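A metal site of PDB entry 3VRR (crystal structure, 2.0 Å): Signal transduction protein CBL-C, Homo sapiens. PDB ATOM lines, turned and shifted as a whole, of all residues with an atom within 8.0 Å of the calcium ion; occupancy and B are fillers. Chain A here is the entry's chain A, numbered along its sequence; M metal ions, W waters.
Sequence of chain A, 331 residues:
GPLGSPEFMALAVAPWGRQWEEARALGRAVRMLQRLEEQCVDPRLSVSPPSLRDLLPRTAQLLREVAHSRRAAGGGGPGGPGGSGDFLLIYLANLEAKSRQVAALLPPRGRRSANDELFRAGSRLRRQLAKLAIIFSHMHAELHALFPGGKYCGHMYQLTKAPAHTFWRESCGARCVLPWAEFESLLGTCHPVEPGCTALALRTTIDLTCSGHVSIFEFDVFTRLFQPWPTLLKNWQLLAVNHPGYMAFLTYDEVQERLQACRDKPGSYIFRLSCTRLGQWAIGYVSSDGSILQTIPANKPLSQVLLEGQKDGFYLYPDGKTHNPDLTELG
Within 4 Å of the calcium ion: Asp 207, Thr 209, Ser 211, His 213 and Glu 218.
OE2 of Glu 218 lies close to N of Leu 208, 3.2 Å away. The side-chain amide nitrogen (ND2) of Asn 94 lies within hydrogen-bond range of the backbone carbonyl oxygen (O) of Thr 209 (2.9 Å). The side-chain carboxylate (OD2) of Asp 207 is in hydrogen-bond range of the backbone NH (N) of Gly 212 (2.8 Å). OG of Ser 215 is in hydrogen-bond range of N of Glu 218, at 3.1 Å. O of Asp 207 lies close to SG of Cys 210, at 3.7 Å.
The calcium ion is bound by the side-chain carboxylate (OD1) of Asp 207 (2.3 Å), the backbone carbonyl oxygen (O) of His 213 (2.4 Å), the side-chain carboxylate (OE2) of Glu 218 (2.4 Å), water W1 (2.5 Å), the side-chain hydroxyl (OG1) of Thr 209 (2.6 Å), the side-chain hydroxyl (OG) of Ser 211 (2.6 Å) and the side-chain carboxylate (OE1) of Glu 218 (2.8 Å). The calcium ion has seven donor atoms within binding distance.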
ATOM      1  N   PHE A  87      11.924   7.393  -4.874  1.00  0.00           N
ATOM      2  CA  PHE A  87      13.371   7.566  -4.783  1.00  0.00           C
ATOM      3  C   PHE A  87      14.047   7.349  -6.177  1.00  0.00           C
ATOM      4  O   PHE A  87      14.882   8.128  -6.627  1.00  0.00           O
ATOM      5  CB  PHE A  87      13.976   6.571  -3.756  1.00  0.00           C
ATOM      6  CG  PHE A  87      15.484   6.712  -3.648  1.00  0.00           C
ATOM      7  CD1 PHE A  87      16.033   7.673  -2.784  1.00  0.00           C
ATOM      8  CD2 PHE A  87      16.328   6.032  -4.527  1.00  0.00           C
ATOM      9  CE1 PHE A  87      17.426   7.865  -2.710  1.00  0.00           C
ATOM     10  CE2 PHE A  87      17.743   6.254  -4.475  1.00  0.00           C
ATOM     11  CZ  PHE A  87      18.275   7.158  -3.527  1.00  0.00           C
ATOM     12  N   ILE A  90      13.340  10.231  -8.663  1.00  0.00           N
ATOM     13  CA  ILE A  90      14.185  11.380  -8.319  1.00  0.00           C
ATOM     14  C   ILE A  90      15.665  11.092  -8.570  1.00  0.00           C
ATOM     15  O   ILE A  90      16.376  11.953  -9.093  1.00  0.00           O
ATOM     16  CB  ILE A  90      13.989  11.786  -6.833  1.00  0.00           C
ATOM     17  CG1 ILE A  90      12.563  12.369  -6.639  1.00  0.00           C
ATOM     18  CG2 ILE A  90      15.118  12.736  -6.365  1.00  0.00           C
ATOM     19  CD1 ILE A  90      11.982  12.053  -5.232  1.00  0.00           C
ATOM     20  N   TYR A  91      16.144   9.910  -8.166  1.00  0.00           N
ATOM     21  CA  TYR A  91      17.568   9.606  -8.303  1.00  0.00           C
ATOM     22  C   TYR A  91      18.008   9.572  -9.783  1.00  0.00           C
ATOM     23  O   TYR A  91      19.027  10.114 -10.137  1.00  0.00           O
ATOM     24  CB  TYR A  91      17.851   8.248  -7.668  1.00  0.00           C
ATOM     25  CG  TYR A  91      19.325   7.792  -7.669  1.00  0.00           C
ATOM     26  CD1 TYR A  91      20.164   8.095  -6.582  1.00  0.00           C
ATOM     27  CD2 TYR A  91      19.854   7.044  -8.716  1.00  0.00           C
ATOM     28  CE1 TYR A  91      21.490   7.693  -6.569  1.00  0.00           C
ATOM     29  CE2 TYR A  91      21.195   6.594  -8.700  1.00  0.00           C
ATOM     30  CZ  TYR A  91      21.992   6.929  -7.606  1.00  0.00           C
ATOM     31  OH  TYR A  91      23.316   6.515  -7.544  1.00  0.00           O
ATOM     32  N   ASN A  94      18.065  13.112 -11.408  1.00  0.00           N
ATOM     33  CA  ASN A  94      19.304  13.715 -11.010  1.00  0.00           C
ATOM     34  C   ASN A  94      20.572  13.078 -11.670  1.00  0.00           C
ATOM     35  O   ASN A  94      21.484  13.807 -12.068  1.00  0.00           O
ATOM     36  CB  ASN A  94      19.464  13.679  -9.509  1.00  0.00           C
ATOM     37  CG  ASN A  94      20.654  14.486  -9.068  1.00  0.00           C
ATOM     38  OD1 ASN A  94      20.789  15.654  -9.442  1.00  0.00           O
ATOM     39  ND2 ASN A  94      21.514  13.899  -8.214  1.00  0.00           N
ATOM     40  N   HIS A 138      28.981  10.445  -3.725  1.00  0.00           N
ATOM     41  CA  HIS A 138      27.767  10.489  -2.885  1.00  0.00           C
ATOM     42  C   HIS A 138      26.548   9.757  -3.463  1.00  0.00           C
ATOM     43  O   HIS A 138      25.871   9.032  -2.762  1.00  0.00           O
ATOM     44  CB  HIS A 138      27.377  11.951  -2.535  1.00  0.00           C
ATOM     45  CG  HIS A 138      28.446  12.702  -1.812  1.00  0.00           C
ATOM     46  ND1 HIS A 138      28.535  14.094  -1.819  1.00  0.00           N
ATOM     47  CD2 HIS A 138      29.516  12.261  -1.106  1.00  0.00           C
ATOM     48  CE1 HIS A 138      29.590  14.457  -1.111  1.00  0.00           C
ATOM     49  NE2 HIS A 138      30.216  13.381  -0.701  1.00  0.00           N
ATOM     50  N   MET A 139      26.263   9.909  -4.739  1.00  0.00           N
ATOM     51  CA  MET A 139      25.125   9.184  -5.343  1.00  0.00           C
ATOM     52  C   MET A 139      25.359   7.660  -5.387  1.00  0.00           C
ATOM     53  O   MET A 139      24.436   6.859  -5.307  1.00  0.00           O
ATOM     54  CB  MET A 139      24.952   9.623  -6.787  1.00  0.00           C
ATOM     55  CG  MET A 139      24.452  11.045  -6.954  1.00  0.00           C
ATOM     56  SD  MET A 139      23.976  11.473  -8.679  1.00  0.00           S
ATOM     57  CE  MET A 139      25.577  11.411  -9.426  1.00  0.00           C
ATOM     58  N   GLU A 142      24.836   6.589  -1.650  1.00  0.00           N
ATOM     59  CA  GLU A 142      23.413   6.617  -1.305  1.00  0.00           C
ATOM     60  C   GLU A 142      22.635   5.427  -1.906  1.00  0.00           C
ATOM     61  O   GLU A 142      21.809   4.776  -1.246  1.00  0.00           O
ATOM     62  CB  GLU A 142      22.838   7.954  -1.777  1.00  0.00           C
ATOM     63  CG  GLU A 142      21.354   8.061  -1.536  1.00  0.00           C
ATOM     64  CD  GLU A 142      20.805   9.364  -2.117  1.00  0.00           C
ATOM     65  OE1 GLU A 142      20.832   9.477  -3.339  1.00  0.00           O
ATOM     66  OE2 GLU A 142      20.352  10.222  -1.335  1.00  0.00           O
ATOM     67  N   VAL A 177      12.901   9.374   1.440  1.00  0.00           N
ATOM     68  CA  VAL A 177      13.274  10.611   0.732  1.00  0.00           C
ATOM     69  C   VAL A 177      12.143  11.672   0.765  1.00  0.00           C
ATOM     70  O   VAL A 177      10.947  11.338   0.806  1.00  0.00           O
ATOM     71  CB  VAL A 177      13.781  10.345  -0.735  1.00  0.00           C
ATOM     72  CG1 VAL A 177      12.651   9.744  -1.652  1.00  0.00           C
ATOM     73  CG2 VAL A 177      14.454  11.598  -1.354  1.00  0.00           C
ATOM     74  N   LEU A 178      12.557  12.912   0.764  1.00  0.00           N
ATOM     75  CA  LEU A 178      11.654  14.064   0.859  1.00  0.00           C
ATOM     76  C   LEU A 178      12.202  15.135  -0.010  1.00  0.00           C
ATOM     77  O   LEU A 178      13.410  15.365   0.015  1.00  0.00           O
ATOM     78  CB  LEU A 178      11.739  14.665   2.298  1.00  0.00           C
ATOM     79  CG  LEU A 178      10.979  14.138   3.539  1.00  0.00           C
ATOM     80  CD1 LEU A 178      10.966  12.639   3.718  1.00  0.00           C
ATOM     81  CD2 LEU A 178      11.604  14.759   4.861  1.00  0.00           C
ATOM     82  N   ARG A 203      20.792  23.695   3.103  1.00  0.00           N
ATOM     83  CA  ARG A 203      20.368  22.783   2.086  1.00  0.00           C
ATOM     84  C   ARG A 203      21.583  22.239   1.304  1.00  0.00           C
ATOM     85  O   ARG A 203      21.646  21.075   1.032  1.00  0.00           O
ATOM     86  CB  ARG A 203      19.361  23.487   1.175  1.00  0.00           C
ATOM     87  CG  ARG A 203      19.060  22.653  -0.071  1.00  0.00           C
ATOM     88  CD  ARG A 203      17.913  23.353  -0.895  1.00  0.00           C
ATOM     89  NE  ARG A 203      17.790  22.773  -2.249  1.00  0.00           N
ATOM     90  CZ  ARG A 203      16.679  22.877  -2.981  1.00  0.00           C
ATOM     91  NH1 ARG A 203      15.649  23.555  -2.500  1.00  0.00           N
ATOM     92  NH2 ARG A 203      16.613  22.359  -4.185  1.00  0.00           N
ATOM     93  N   ILE A 206      23.472  19.582   3.361  1.00  0.00           N
ATOM     94  CA  ILE A 206      22.782  18.306   3.610  1.00  0.00           C
ATOM     95  C   ILE A 206      22.597  17.535   2.290  1.00  0.00           C
ATOM     96  O   ILE A 206      22.697  16.278   2.239  1.00  0.00           O
ATOM     97  CB  ILE A 206      21.429  18.534   4.324  1.00  0.00           C
ATOM     98  CG1 ILE A 206      21.605  19.030   5.780  1.00  0.00           C
ATOM     99  CG2 ILE A 206      20.532  17.285   4.277  1.00  0.00           C
ATOM    100  CD1 ILE A 206      20.249  19.421   6.457  1.00  0.00           C
ATOM    101  N   ASP A 207      22.369  18.298   1.220  1.00  0.00           N
ATOM    102  CA  ASP A 207      22.065  17.694  -0.083  1.00  0.00           C
ATOM    103  C   ASP A 207      23.359  17.278  -0.791  1.00  0.00           C
ATOM    104  O   ASP A 207      23.781  17.906  -1.794  1.00  0.00           O
ATOM    105  CB  ASP A 207      21.251  18.681  -0.939  1.00  0.00           C
ATOM    106  CG  ASP A 207      20.773  18.072  -2.281  1.00  0.00           C
ATOM    107  OD1 ASP A 207      20.861  16.859  -2.477  1.00  0.00           O
ATOM    108  OD2 ASP A 207      20.391  18.848  -3.164  1.00  0.00           O
ATOM    109  N   LEU A 208      23.944  16.174  -0.317  1.00  0.00           N
ATOM    110  CA  LEU A 208      25.188  15.655  -0.871  1.00  0.00           C
ATOM    111  C   LEU A 208      25.104  15.303  -2.378  1.00  0.00           C
ATOM    112  O   LEU A 208      26.091  15.432  -3.118  1.00  0.00           O
ATOM    113  CB  LEU A 208      25.579  14.371  -0.095  1.00  0.00           C
ATOM    114  CG  LEU A 208      25.660  14.386   1.433  1.00  0.00           C
ATOM    115  CD1 LEU A 208      26.150  12.962   1.879  1.00  0.00           C
ATOM    116  CD2 LEU A 208      26.611  15.460   1.943  1.00  0.00           C
ATOM    117  N   THR A 209      23.946  14.814  -2.811  1.00  0.00           N
ATOM    118  CA  THR A 209      23.796  14.426  -4.222  1.00  0.00           C
ATOM    119  C   THR A 209      23.350  15.600  -5.139  1.00  0.00           C
ATOM    120  O   THR A 209      23.245  15.438  -6.388  1.00  0.00           O
ATOM    121  CB  THR A 209      22.814  13.220  -4.386  1.00  0.00           C
ATOM    122  OG1 THR A 209      21.502  13.600  -4.000  1.00  0.00           O
ATOM    123  CG2 THR A 209      23.246  11.961  -3.524  1.00  0.00           C
ATOM    124  N   CYS A 210      23.104  16.757  -4.507  1.00  0.00           N
ATOM    125  CA  CYS A 210      22.694  17.972  -5.150  1.00  0.00           C
ATOM    126  C   CYS A 210      21.450  17.740  -5.988  1.00  0.00           C
ATOM    127  O   CYS A 210      21.366  18.225  -7.145  1.00  0.00           O
ATOM    128  CB  CYS A 210      23.853  18.555  -5.994  1.00  0.00           C
ATOM    129  SG  CYS A 210      25.246  19.065  -5.041  1.00  0.00           S
ATOM    130  N   SER A 211      20.543  16.909  -5.488  1.00  0.00           N
ATOM    131  CA  SER A 211      19.331  16.499  -6.196  1.00  0.00           C
ATOM    132  C   SER A 211      18.084  17.292  -5.837  1.00  0.00           C
ATOM    133  O   SER A 211      17.041  17.041  -6.429  1.00  0.00           O
ATOM    134  CB  SER A 211      19.016  15.023  -5.879  1.00  0.00           C
ATOM    135  OG  SER A 211      18.665  14.903  -4.496  1.00  0.00           O
ATOM    136  N   GLY A 212      18.196  18.193  -4.851  1.00  0.00           N
ATOM    137  CA  GLY A 212      17.058  18.969  -4.325  1.00  0.00           C
ATOM    138  C   GLY A 212      16.204  18.205  -3.332  1.00  0.00           C
ATOM    139  O   GLY A 212      15.163  18.696  -2.926  1.00  0.00           O
ATOM    140  N   HIS A 213      16.593  16.962  -3.016  1.00  0.00           N
ATOM    141  CA  HIS A 213      15.806  16.074  -2.153  1.00  0.00           C
ATOM    142  C   HIS A 213      16.729  15.555  -1.070  1.00  0.00           C
ATOM    143  O   HIS A 213      17.942  15.488  -1.276  1.00  0.00           O
ATOM    144  CB  HIS A 213      15.266  14.912  -2.964  1.00  0.00           C
ATOM    145  CG  HIS A 213      14.312  15.355  -4.024  1.00  0.00           C
ATOM    146  ND1 HIS A 213      14.691  16.196  -5.054  1.00  0.00           N
ATOM    147  CD2 HIS A 213      12.969  15.224  -4.114  1.00  0.00           C
ATOM    148  CE1 HIS A 213      13.627  16.489  -5.786  1.00  0.00           C
ATOM    149  NE2 HIS A 213      12.578  15.900  -5.240  1.00  0.00           N
ATOM    150  N   VAL A 214      16.158  15.269   0.105  1.00  0.00           N
ATOM    151  CA  VAL A 214      16.951  14.748   1.212  1.00  0.00           C
ATOM    152  C   VAL A 214      16.561  13.294   1.432  1.00  0.00           C
ATOM    153  O   VAL A 214      15.380  13.026   1.784  1.00  0.00           O
ATOM    154  CB  VAL A 214      16.692  15.541   2.498  1.00  0.00           C
ATOM    155  CG1 VAL A 214      17.530  14.948   3.707  1.00  0.00           C
ATOM    156  CG2 VAL A 214      16.991  17.060   2.264  1.00  0.00           C
ATOM    157  N   SER A 215      17.512  12.351   1.189  1.00  0.00           N
ATOM    158  CA  SER A 215      17.240  10.982   1.589  1.00  0.00           C
ATOM    159  C   SER A 215      17.480  10.699   3.080  1.00  0.00           C
ATOM    160  O   SER A 215      18.187  11.439   3.730  1.00  0.00           O
ATOM    161  CB  SER A 215      18.038   9.985   0.787  1.00  0.00           C
ATOM    162  OG  SER A 215      19.432  10.140   1.050  1.00  0.00           O
ATOM    163  N   GLU A 218      21.284  10.686   3.484  1.00  0.00           N
ATOM    164  CA  GLU A 218      21.822  12.035   3.624  1.00  0.00           C
ATOM    165  C   GLU A 218      21.582  12.570   5.022  1.00  0.00           C
ATOM    166  O   GLU A 218      22.485  13.210   5.650  1.00  0.00           O
ATOM    167  CB  GLU A 218      21.198  12.979   2.595  1.00  0.00           C
ATOM    168  CG  GLU A 218      21.935  12.866   1.256  1.00  0.00           C
ATOM    169  CD  GLU A 218      21.155  13.532   0.148  1.00  0.00           C
ATOM    170  OE1 GLU A 218      19.921  13.657   0.287  1.00  0.00           O
ATOM    171  OE2 GLU A 218      21.768  13.958  -0.848  1.00  0.00           O
HETATM  172 CA    CA M   1      19.986  14.733  -2.255  1.00  0.00          CA
HETATM  173  O   HOH W   1      19.063  12.428  -2.052  1.00  0.00           O
